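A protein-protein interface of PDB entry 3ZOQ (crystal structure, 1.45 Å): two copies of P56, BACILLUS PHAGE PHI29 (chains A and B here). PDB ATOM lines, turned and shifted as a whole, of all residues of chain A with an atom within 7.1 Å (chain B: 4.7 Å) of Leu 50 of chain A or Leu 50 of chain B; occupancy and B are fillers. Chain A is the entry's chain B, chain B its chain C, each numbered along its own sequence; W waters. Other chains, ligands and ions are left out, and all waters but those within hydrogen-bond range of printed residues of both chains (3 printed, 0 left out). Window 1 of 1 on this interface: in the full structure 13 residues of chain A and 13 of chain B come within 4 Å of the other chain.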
ATOM      1  N   TYR A  10     -23.326  -2.751  -4.251  1.00  0.00           N
ATOM      2  CA  TYR A  10     -21.923  -2.863  -4.638  1.00  0.00           C
ATOM      3  C   TYR A  10     -21.021  -1.926  -3.845  1.00  0.00           C
ATOM      4  O   TYR A  10     -21.418  -0.812  -3.487  1.00  0.00           O
ATOM      5  CB  TYR A  10     -21.758  -2.535  -6.137  1.00  0.00           C
ATOM      6  CG  TYR A  10     -22.333  -3.605  -7.040  1.00  0.00           C
ATOM      7  CD1 TYR A  10     -23.698  -3.660  -7.304  1.00  0.00           C
ATOM      8  CD2 TYR A  10     -21.513  -4.575  -7.607  1.00  0.00           C
ATOM      9  CE1 TYR A  10     -24.234  -4.652  -8.107  1.00  0.00           C
ATOM     10  CE2 TYR A  10     -22.037  -5.572  -8.415  1.00  0.00           C
ATOM     11  CZ  TYR A  10     -23.399  -5.597  -8.668  1.00  0.00           C
ATOM     12  OH  TYR A  10     -23.925  -6.585  -9.470  1.00  0.00           O
ATOM     13  N   VAL A  12     -17.485   0.160  -4.375  1.00  0.00           N
ATOM     14  CA  VAL A  12     -16.688   0.670  -5.497  1.00  0.00           C
ATOM     15  C   VAL A  12     -15.396   1.244  -4.970  1.00  0.00           C
ATOM     16  O   VAL A  12     -15.417   2.161  -4.143  1.00  0.00           O
ATOM     17  CB  VAL A  12     -17.429   1.798  -6.258  1.00  0.00           C
ATOM     18  CG1 VAL A  12     -16.638   2.246  -7.483  1.00  0.00           C
ATOM     19  CG2 VAL A  12     -18.831   1.359  -6.649  1.00  0.00           C
ATOM     20  N   THR A  13     -14.279   0.722  -5.473  1.00  0.00           N
ATOM     21  CA  THR A  13     -12.967   1.218  -5.096  1.00  0.00           C
ATOM     22  C   THR A  13     -12.279   1.762  -6.337  1.00  0.00           C
ATOM     23  O   THR A  13     -12.270   1.120  -7.388  1.00  0.00           O
ATOM     24  CB  THR A  13     -12.125   0.117  -4.434  1.00  0.00           C
ATOM     25  OG1 THR A  13     -12.828  -0.346  -3.278  1.00  0.00           O
ATOM     26  CG2 THR A  13     -10.754   0.650  -4.023  1.00  0.00           C
ATOM     27  N   MET A  14     -11.716   2.953  -6.219  1.00  0.00           N
ATOM     28  CA  MET A  14     -10.956   3.522  -7.326  1.00  0.00           C
ATOM     29  C   MET A  14      -9.589   4.010  -6.887  1.00  0.00           C
ATOM     30  O   MET A  14      -9.462   4.610  -5.817  1.00  0.00           O
ATOM     31  CB  MET A  14     -11.726   4.674  -7.962  1.00  0.00           C
ATOM     32  CG  MET A  14     -12.950   4.205  -8.722  1.00  0.00           C
ATOM     33  SD  MET A  14     -13.832   5.529  -9.552  1.00  0.00           S
ATOM     34  CE  MET A  14     -14.603   6.309  -8.145  1.00  0.00           C
ATOM     35  N   LEU A  15      -8.576   3.728  -7.712  1.00  0.00           N
ATOM     36  CA  LEU A  15      -7.270   4.377  -7.601  1.00  0.00           C
ATOM     37  C   LEU A  15      -7.258   5.493  -8.637  1.00  0.00           C
ATOM     38  O   LEU A  15      -7.399   5.229  -9.833  1.00  0.00           O
ATOM     39  CB  LEU A  15      -6.121   3.382  -7.843  1.00  0.00           C
ATOM     40  CG  LEU A  15      -4.700   3.951  -7.765  1.00  0.00           C
ATOM     41  CD1 LEU A  15      -4.433   4.483  -6.367  1.00  0.00           C
ATOM     42  CD2 LEU A  15      -3.661   2.885  -8.098  1.00  0.00           C
ATOM     43  N   TYR A  25      -6.444   6.155  -3.339  1.00  0.00           N
ATOM     44  CA  TYR A  25      -7.672   5.352  -3.368  1.00  0.00           C
ATOM     45  C   TYR A  25      -8.891   6.095  -2.781  1.00  0.00           C
ATOM     46  O   TYR A  25      -8.768   6.815  -1.798  1.00  0.00           O
ATOM     47  CB  TYR A  25      -7.454   4.028  -2.599  1.00  0.00           C
ATOM     48  CG  TYR A  25      -6.772   2.912  -3.373  1.00  0.00           C
ATOM     49  CD1 TYR A  25      -7.484   2.157  -4.303  1.00  0.00           C
ATOM     50  CD2 TYR A  25      -5.424   2.584  -3.150  1.00  0.00           C
ATOM     51  CE1 TYR A  25      -6.881   1.129  -5.016  1.00  0.00           C
ATOM     52  CE2 TYR A  25      -4.807   1.548  -3.860  1.00  0.00           C
ATOM     53  CZ  TYR A  25      -5.545   0.822  -4.789  1.00  0.00           C
ATOM     54  OH  TYR A  25      -4.959  -0.209  -5.504  1.00  0.00           O
ATOM     55  N   PHE A  36     -23.480   3.615  -9.169  1.00  0.00           N
ATOM     56  CA  PHE A  36     -22.117   3.444  -9.667  1.00  0.00           C
ATOM     57  C   PHE A  36     -21.920   4.182 -11.006  1.00  0.00           C
ATOM     58  O   PHE A  36     -20.908   4.854 -11.207  1.00  0.00           O
ATOM     59  CB  PHE A  36     -21.754   1.956  -9.808  1.00  0.00           C
ATOM     60  CG  PHE A  36     -20.581   1.717 -10.723  1.00  0.00           C
ATOM     61  CD1 PHE A  36     -19.309   2.184 -10.367  1.00  0.00           C
ATOM     62  CD2 PHE A  36     -20.754   1.090 -11.959  1.00  0.00           C
ATOM     63  CE1 PHE A  36     -18.225   2.002 -11.216  1.00  0.00           C
ATOM     64  CE2 PHE A  36     -19.670   0.899 -12.808  1.00  0.00           C
ATOM     65  CZ  PHE A  36     -18.409   1.354 -12.433  1.00  0.00           C
ATOM     66  N   TYR A  40     -19.232   7.172 -11.583  1.00  0.00           N
ATOM     67  CA  TYR A  40     -18.201   7.146 -12.623  1.00  0.00           C
ATOM     68  C   TYR A  40     -18.187   8.476 -13.397  1.00  0.00           C
ATOM     69  O   TYR A  40     -17.120   9.093 -13.613  1.00  0.00           O
ATOM     70  CB  TYR A  40     -18.472   5.969 -13.545  1.00  0.00           C
ATOM     71  CG  TYR A  40     -17.480   5.769 -14.668  1.00  0.00           C
ATOM     72  CD1 TYR A  40     -16.267   5.108 -14.448  1.00  0.00           C
ATOM     73  CD2 TYR A  40     -17.785   6.163 -15.970  1.00  0.00           C
ATOM     74  CE1 TYR A  40     -15.370   4.883 -15.492  1.00  0.00           C
ATOM     75  CE2 TYR A  40     -16.897   5.939 -17.016  1.00  0.00           C
ATOM     76  CZ  TYR A  40     -15.696   5.295 -16.768  1.00  0.00           C
ATOM     77  OH  TYR A  40     -14.811   5.055 -17.792  1.00  0.00           O
ATOM     78  N   THR A  43     -16.529  11.420 -11.420  1.00  0.00           N
ATOM     79  CA  THR A  43     -15.126  11.219 -11.033  1.00  0.00           C
ATOM     80  C   THR A  43     -14.223  12.046 -11.948  1.00  0.00           C
ATOM     81  O   THR A  43     -14.056  11.700 -13.124  1.00  0.00           O
ATOM     82  CB  THR A  43     -14.778   9.719 -11.084  1.00  0.00           C
ATOM     83  OG1 THR A  43     -15.617   9.021 -10.152  1.00  0.00           O
ATOM     84  CG2 THR A  43     -13.315   9.478 -10.730  1.00  0.00           C
ATOM     85  N   ILE A  47      -8.685   7.897 -13.861  1.00  0.00           N
ATOM     86  CA  ILE A  47      -8.892   6.578 -13.246  1.00  0.00           C
ATOM     87  C   ILE A  47      -7.729   5.655 -13.605  1.00  0.00           C
ATOM     88  O   ILE A  47      -7.474   5.362 -14.783  1.00  0.00           O
ATOM     89  CB  ILE A  47     -10.244   5.940 -13.653  1.00  0.00           C
ATOM     90  CG1 ILE A  47     -11.401   6.843 -13.185  1.00  0.00           C
ATOM     91  CG2 ILE A  47     -10.362   4.513 -13.104  1.00  0.00           C
ATOM     92  CD1 ILE A  47     -12.755   6.455 -13.741  1.00  0.00           C
ATOM     93  N   ILE A  48      -7.006   5.211 -12.581  1.00  0.00           N
ATOM     94  CA  ILE A  48      -5.909   4.255 -12.762  1.00  0.00           C
ATOM     95  C   ILE A  48      -6.405   2.821 -12.575  1.00  0.00           C
ATOM     96  O   ILE A  48      -6.069   1.929 -13.367  1.00  0.00           O
ATOM     97  CB  ILE A  48      -4.745   4.565 -11.793  1.00  0.00           C
ATOM     98  CG1 ILE A  48      -4.308   6.042 -11.922  1.00  0.00           C
ATOM     99  CG2 ILE A  48      -3.582   3.604 -12.007  1.00  0.00           C
ATOM    100  CD1 ILE A  48      -3.847   6.444 -13.315  1.00  0.00           C
ATOM    101  N   LYS A  49      -7.165   2.584 -11.501  1.00  0.00           N
ATOM    102  CA  LYS A  49      -7.804   1.285 -11.285  1.00  0.00           C
ATOM    103  C   LYS A  49      -9.225   1.507 -10.798  1.00  0.00           C
ATOM    104  O   LYS A  49      -9.510   2.477 -10.104  1.00  0.00           O
ATOM    105  CB  LYS A  49      -7.045   0.419 -10.267  1.00  0.00           C
ATOM    106  CG  LYS A  49      -5.613   0.087 -10.665  1.00  0.00           C
ATOM    107  CD  LYS A  49      -4.932  -0.784  -9.610  1.00  0.00           C
ATOM    108  CE  LYS A  49      -3.487  -1.098  -9.978  1.00  0.00           C
ATOM    109  NZ  LYS A  49      -3.344  -1.815 -11.285  1.00  0.00           N
ATOM    110  N   LEU A  50     -10.112   0.588 -11.156  1.00  0.00           N
ATOM    111  CA  LEU A  50     -11.480   0.609 -10.659  1.00  0.00           C
ATOM    112  C   LEU A  50     -11.885  -0.814 -10.299  1.00  0.00           C
ATOM    113  O   LEU A  50     -11.600  -1.763 -11.041  1.00  0.00           O
ATOM    114  CB  LEU A  50     -12.404   1.214 -11.728  1.00  0.00           C
ATOM    115  CG  LEU A  50     -13.890   1.401 -11.401  1.00  0.00           C
ATOM    116  CD1 LEU A  50     -14.429   2.578 -12.198  1.00  0.00           C
ATOM    117  CD2 LEU A  50     -14.642   0.118 -11.716  1.00  0.00           C
ATOM    118  N   ARG A  51     -12.551  -0.964  -9.157  1.00  0.00           N
ATOM    119  CA  ARG A  51     -13.033  -2.261  -8.705  1.00  0.00           C
ATOM    120  C   ARG A  51     -14.488  -2.135  -8.291  1.00  0.00           C
ATOM    121  O   ARG A  51     -14.853  -1.205  -7.568  1.00  0.00           O
ATOM    122  CB  ARG A  51     -12.201  -2.771  -7.528  1.00  0.00           C
ATOM    123  CG  ARG A  51     -10.711  -2.843  -7.833  1.00  0.00           C
ATOM    124  CD  ARG A  51      -9.868  -3.170  -6.616  1.00  0.00           C
ATOM    125  NE  ARG A  51      -9.958  -4.584  -6.267  1.00  0.00           N
ATOM    126  CZ  ARG A  51      -9.270  -5.560  -6.858  1.00  0.00           C
ATOM    127  NH1 ARG A  51      -8.424  -5.295  -7.852  1.00  0.00           N
ATOM    128  NH2 ARG A  51      -9.437  -6.811  -6.457  1.00  0.00           N
ATOM    129  N   LEU A  52     -15.308  -3.056  -8.781  1.00  0.00           N
ATOM    130  CA  LEU A  52     -16.711  -3.133  -8.414  1.00  0.00           C
ATOM    131  C   LEU A  52     -16.859  -4.518  -7.816  1.00  0.00           C
ATOM    132  O   LEU A  52     -16.377  -5.500  -8.384  1.00  0.00           O
ATOM    133  CB  LEU A  52     -17.564  -2.957  -9.676  1.00  0.00           C
ATOM    134  CG  LEU A  52     -19.089  -2.887  -9.698  1.00  0.00           C
ATOM    135  CD1 LEU A  52     -19.612  -1.774  -8.808  1.00  0.00           C
ATOM    136  CD2 LEU A  52     -19.504  -2.665 -11.145  1.00  0.00           C
ATOM    137  N   ASP A  53     -17.457  -4.589  -6.632  1.00  0.00           N
ATOM    138  CA  ASP A  53     -17.666  -5.870  -5.947  1.00  0.00           C
ATOM    139  C   ASP A  53     -19.076  -5.925  -5.384  1.00  0.00           C
ATOM    140  O   ASP A  53     -19.470  -5.063  -4.585  1.00  0.00           O
ATOM    141  CB  ASP A  53     -16.650  -6.068  -4.808  1.00  0.00           C
ATOM    142  CG  ASP A  53     -15.225  -6.295  -5.313  1.00  0.00           C
ATOM    143  OD1 ASP A  53     -14.532  -5.313  -5.664  1.00  0.00           O
ATOM    144  OD2 ASP A  53     -14.782  -7.464  -5.334  1.00  0.00           O
ATOM    145  N   LYS A  54     -19.840  -6.932  -5.802  1.00  0.00           N
ATOM    146  CA  LYS A  54     -21.167  -7.157  -5.252  1.00  0.00           C
ATOM    147  C   LYS A  54     -21.065  -7.502  -3.777  1.00  0.00           C
ATOM    148  O   LYS A  54     -20.244  -8.338  -3.383  1.00  0.00           O
ATOM    149  CB  LYS A  54     -21.873  -8.289  -6.004  1.00  0.00           C
ATOM    150  CG  LYS A  54     -23.324  -8.486  -5.597  1.00  0.00           C
ATOM    151  CD  LYS A  54     -23.960  -9.667  -6.311  1.00  0.00           C
ATOM    152  CE  LYS A  54     -25.351  -9.931  -5.747  1.00  0.00           C
ATOM    153  NZ  LYS A  54     -25.992 -11.124  -6.364  1.00  0.00           N
ATOM    154  N   THR B  13     -11.185  -7.372 -16.221  1.00  0.00           N
ATOM    155  CA  THR B  13     -11.591  -8.712 -15.805  1.00  0.00           C
ATOM    156  C   THR B  13     -12.965  -8.615 -15.154  1.00  0.00           C
ATOM    157  O   THR B  13     -13.209  -7.727 -14.351  1.00  0.00           O
ATOM    158  CB  THR B  13     -10.592  -9.316 -14.802  1.00  0.00           C
ATOM    159  OG1 THR B  13      -9.321  -9.471 -15.440  1.00  0.00           O
ATOM    160  CG2 THR B  13     -11.074 -10.675 -14.294  1.00  0.00           C
ATOM    161  N   MET B  14     -13.861  -9.522 -15.509  1.00  0.00           N
ATOM    162  CA  MET B  14     -15.148  -9.606 -14.833  1.00  0.00           C
ATOM    163  C   MET B  14     -15.431 -11.027 -14.386  1.00  0.00           C
ATOM    164  O   MET B  14     -15.181 -11.990 -15.121  1.00  0.00           O
ATOM    165  CB  MET B  14     -16.279  -9.118 -15.743  1.00  0.00           C
ATOM    166  CG  MET B  14     -16.180  -7.641 -16.087  1.00  0.00           C
ATOM    167  SD  MET B  14     -17.547  -7.080 -17.108  1.00  0.00           S
ATOM    168  CE  MET B  14     -17.095  -7.747 -18.705  1.00  0.00           C
ATOM    169  N   PHE B  36     -14.049   0.191 -22.821  1.00  0.00           N
ATOM    170  CA  PHE B  36     -14.496  -0.325 -21.533  1.00  0.00           C
ATOM    171  C   PHE B  36     -15.957   0.072 -21.254  1.00  0.00           C
ATOM    172  O   PHE B  36     -16.771  -0.753 -20.823  1.00  0.00           O
ATOM    173  CB  PHE B  36     -13.577   0.164 -20.414  1.00  0.00           C
ATOM    174  CG  PHE B  36     -14.218   0.124 -19.047  1.00  0.00           C
ATOM    175  CD1 PHE B  36     -14.565  -1.110 -18.472  1.00  0.00           C
ATOM    176  CD2 PHE B  36     -14.523   1.308 -18.358  1.00  0.00           C
ATOM    177  CE1 PHE B  36     -15.171  -1.163 -17.223  1.00  0.00           C
ATOM    178  CE2 PHE B  36     -15.141   1.255 -17.105  1.00  0.00           C
ATOM    179  CZ  PHE B  36     -15.463   0.015 -16.545  1.00  0.00           C
ATOM    180  N   TYR B  40     -19.057  -2.484 -20.774  1.00  0.00           N
ATOM    181  CA  TYR B  40     -19.920  -2.476 -19.591  1.00  0.00           C
ATOM    182  C   TYR B  40     -21.401  -2.503 -19.984  1.00  0.00           C
ATOM    183  O   TYR B  40     -22.169  -3.319 -19.470  1.00  0.00           O
ATOM    184  CB  TYR B  40     -19.609  -1.258 -18.715  1.00  0.00           C
ATOM    185  CG  TYR B  40     -20.542  -1.099 -17.533  1.00  0.00           C
ATOM    186  CD1 TYR B  40     -20.318  -1.789 -16.346  1.00  0.00           C
ATOM    187  CD2 TYR B  40     -21.660  -0.253 -17.604  1.00  0.00           C
ATOM    188  CE1 TYR B  40     -21.177  -1.637 -15.258  1.00  0.00           C
ATOM    189  CE2 TYR B  40     -22.527  -0.107 -16.525  1.00  0.00           C
ATOM    190  CZ  TYR B  40     -22.280  -0.801 -15.354  1.00  0.00           C
ATOM    191  OH  TYR B  40     -23.130  -0.660 -14.264  1.00  0.00           O
ATOM    192  N   ILE B  47     -23.020  -8.836 -12.826  1.00  0.00           N
ATOM    193  CA  ILE B  47     -21.641  -8.582 -12.404  1.00  0.00           C
ATOM    194  C   ILE B  47     -21.444  -8.961 -10.933  1.00  0.00           C
ATOM    195  O   ILE B  47     -22.112  -8.410 -10.046  1.00  0.00           O
ATOM    196  CB  ILE B  47     -21.223  -7.107 -12.640  1.00  0.00           C
ATOM    197  CG1 ILE B  47     -21.271  -6.758 -14.137  1.00  0.00           C
ATOM    198  CG2 ILE B  47     -19.814  -6.851 -12.101  1.00  0.00           C
ATOM    199  CD1 ILE B  47     -21.102  -5.282 -14.447  1.00  0.00           C
ATOM    200  N   ILE B  48     -20.540  -9.903 -10.674  1.00  0.00           N
ATOM    201  CA  ILE B  48     -20.137 -10.232  -9.304  1.00  0.00           C
ATOM    202  C   ILE B  48     -18.875  -9.436  -8.943  1.00  0.00           C
ATOM    203  O   ILE B  48     -18.807  -8.803  -7.874  1.00  0.00           O
ATOM    204  CB  ILE B  48     -19.911 -11.755  -9.099  1.00  0.00           C
ATOM    205  CG1 ILE B  48     -21.111 -12.584  -9.598  1.00  0.00           C
ATOM    206  CG2 ILE B  48     -19.606 -12.070  -7.637  1.00  0.00           C
ATOM    207  CD1 ILE B  48     -22.436 -12.254  -8.934  1.00  0.00           C
ATOM    208  N   LYS B  49     -17.885  -9.458  -9.843  1.00  0.00           N
ATOM    209  CA  LYS B  49     -16.679  -8.635  -9.710  1.00  0.00           C
ATOM    210  C   LYS B  49     -16.351  -7.981 -11.053  1.00  0.00           C
ATOM    211  O   LYS B  49     -16.540  -8.577 -12.107  1.00  0.00           O
ATOM    212  CB  LYS B  49     -15.467  -9.464  -9.254  1.00  0.00           C
ATOM    213  CG  LYS B  49     -15.607 -10.122  -7.885  1.00  0.00           C
ATOM    214  CD  LYS B  49     -14.474 -11.100  -7.620  1.00  0.00           C
ATOM    215  CE  LYS B  49     -14.645 -11.773  -6.264  1.00  0.00           C
ATOM    216  NZ  LYS B  49     -13.657 -12.866  -6.030  1.00  0.00           N
ATOM    217  N   LEU B  50     -15.875  -6.752 -11.011  1.00  0.00           N
ATOM    218  CA  LEU B  50     -15.340  -6.096 -12.195  1.00  0.00           C
ATOM    219  C   LEU B  50     -14.050  -5.390 -11.783  1.00  0.00           C
ATOM    220  O   LEU B  50     -13.984  -4.753 -10.730  1.00  0.00           O
ATOM    221  CB  LEU B  50     -16.363  -5.125 -12.791  1.00  0.00           C
ATOM    222  CG  LEU B  50     -15.933  -4.278 -14.001  1.00  0.00           C
ATOM    223  CD1 LEU B  50     -17.130  -3.942 -14.878  1.00  0.00           C
ATOM    224  CD2 LEU B  50     -15.189  -3.014 -13.590  1.00  0.00           C
ATOM    225  N   ARG B  51     -13.012  -5.559 -12.595  1.00  0.00           N
ATOM    226  CA  ARG B  51     -11.727  -4.895 -12.386  1.00  0.00           C
ATOM    227  C   ARG B  51     -11.285  -4.224 -13.684  1.00  0.00           C
ATOM    228  O   ARG B  51     -11.289  -4.849 -14.757  1.00  0.00           O
ATOM    229  CB  ARG B  51     -10.656  -5.898 -11.918  1.00  0.00           C
ATOM    230  CG  ARG B  51     -10.795  -6.357 -10.466  1.00  0.00           C
ATOM    231  CD  ARG B  51     -11.741  -7.540 -10.344  1.00  0.00           C
ATOM    232  NE  ARG B  51     -11.821  -8.060  -8.977  1.00  0.00           N
ATOM    233  CZ  ARG B  51     -12.558  -7.526  -8.000  1.00  0.00           C
ATOM    234  NH1 ARG B  51     -13.291  -6.440  -8.213  1.00  0.00           N
ATOM    235  NH2 ARG B  51     -12.553  -8.086  -6.797  1.00  0.00           N
ATOM    236  N   LEU B  52     -10.913  -2.957 -13.571  1.00  0.00           N
ATOM    237  CA  LEU B  52     -10.347  -2.172 -14.660  1.00  0.00           C
ATOM    238  C   LEU B  52      -8.963  -1.757 -14.201  1.00  0.00           C
ATOM    239  O   LEU B  52      -8.826  -1.177 -13.121  1.00  0.00           O
ATOM    240  CB  LEU B  52     -11.197  -0.915 -14.916  1.00  0.00           C
ATOM    241  CG  LEU B  52     -10.681   0.115 -15.928  1.00  0.00           C
ATOM    242  CD1 LEU B  52     -10.818  -0.426 -17.354  1.00  0.00           C
ATOM    243  CD2 LEU B  52     -11.434   1.434 -15.763  1.00  0.00           C
HETATM  244  O   HOH W   1     -18.547  -9.916  -5.018  1.00  0.00           O
HETATM  245  O   HOH W   2     -11.746  -5.517  -4.801  1.00  0.00           O
HETATM  246  O   HOH W   3      -8.530  -3.002 -10.512  1.00  0.00           O
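Lys 49 of chain A touches Leu 52 of chain B, and with the chains exchanged Leu 52 of chain A touches Lys 49 of chain B.
Leu 50 of chain B touches its own counterpart, Leu 50 of chain A.
Leu 50 of chain A touches Arg 51 of chain B, and with the chains exchanged Arg 51 of chain A touches Leu 50 of chain B.
Leu 50 of chain A touches Leu 52 of chain B, and with the chains exchanged Leu 52 of chain A touches Leu 50 of chain B.
10 positions are printed for both chains.
The backbone carbonyl oxygen (O) of Thr 13 of chain A lies within hydrogen-bond range of the backbone NH (N) of Arg 51 of chain A (2.7 Å).
The backbone NH (N) of Leu 15 of chain A is in hydrogen-bond range of the backbone carbonyl oxygen (O) of Lys 49 of chain A, 2.9 Å away.
The backbone carbonyl oxygen (O) of Thr 13 of chain B sits at hydrogen-bond distance from the backbone NH (N) of Arg 51 of chain B (2.8 Å).
Water W2 lies within hydrogen-bond range of the guanidinium group (NE) of Arg 51 of chain A (2.5 Å), the side-chain carboxylate (OD1) of Asp 53 of chain A (2.9 Å) and the guanidinium group (NH2) of Arg 51 of chain B (3.4 Å).
Water W1 lies within hydrogen-bond range of O of Lys 54 of chain A (2.8 Å) and O of Ile 48 of chain B (3.1 Å).
Water W3 lies within hydrogen-bond range of the backbone carbonyl oxygen of Leu 52 of chain B and the backbone carbonyl oxygen of Leu 50 of chain A.
Of the printed residues of chain B, Leu 50 of chain A touches Leu 50 (3.7 Å), Arg 51 (3.4 Å) and Leu 52 (2.9 Å).
Of the printed residues of chain A, Tyr 40 of chain B touches Phe 36.
Printed residues of chain A within 4 Å of Lys 49 of chain B: Leu 52 (3.4 Å) and Asp 53 (3.8 Å).
Printed residues of chain A within 4 Å of Leu 50 of chain B: Leu 50, Arg 51 and Leu 52.
The nearest printed residue of chain B that does not touch Leu 50 of chain A is Phe 36 of chain B (4.9 Å).
Printed residues of chain A that touch a printed residue of chain B: Tyr 10, Phe 36, Tyr 40, Lys 49, Leu 50, Arg 51, Leu 52, Asp 53 and Lys 54.
Hydrophobic or aromatic side chains of chain A within 4 Å of the printed part of chain B: Tyr 10, Phe 36, Tyr 40, Leu 50 and Leu 52.
Among the printed residues, Asp or Glu carboxylates within 4 Å of a Lys or Arg side-chain nitrogen of the other chain: Asp 53 of chain A with Arg 51 of chain B (2.7 Å).
The backbone carbonyl oxygen (O) of Ile 47 of chain B lies within hydrogen-bond range of the side-chain hydroxyl (OH) of Tyr 10 of chain A, at 2.6 Å.
O of Leu 50 of chain A lies within hydrogen-bond range of N of Leu 52 of chain B (2.9 Å).
N of Leu 52 of chain A is in hydrogen-bond range of O of Leu 50 of chain B.
NH1 of Arg 51 of chain B lies within hydrogen-bond range of O of Leu 52 of chain A (3.2 Å).
The side-chain carboxylate (OD2) of Asp 53 of chain A lies within salt-bridge range of the guanidinium group (NH2) of Arg 51 of chain B, at 2.7 Å.
The backbone carbonyl oxygen (O) of Ile 48 of chain B sits at hydrogen-bond distance from the backbone NH (N) of Lys 54 of chain A.
NH2 of Arg 51 of chain B lies close to NH2 of Arg 51 of chain A (3.4 Å).
OH of Tyr 40 of chain B touches CD2 of Phe 36 of chain A, at 3.7 Å.
Phe 36 of chain B touches Tyr 40 of chain A.
Lys 49 of chain A touches Leu 52 of chain B.
Leu 50 of chain A touches Leu 50 of chain B (CD2 to CD2, 3.7 Å).
Arg 51 of chain B touches Leu 50 of chain A (CA to O, 3.4 Å).
CA of Arg 51 of chain A touches O of Leu 50 of chain B, 3.3 Å away.
O of Leu 52 of chain A touches CA of Lys 49 of chain B, at 3.4 Å.
Asp 53 of chain A touches Ile 48 of chain B.
OD2 of Asp 53 of chain A touches CG of Lys 49 of chain B (3.8 Å).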
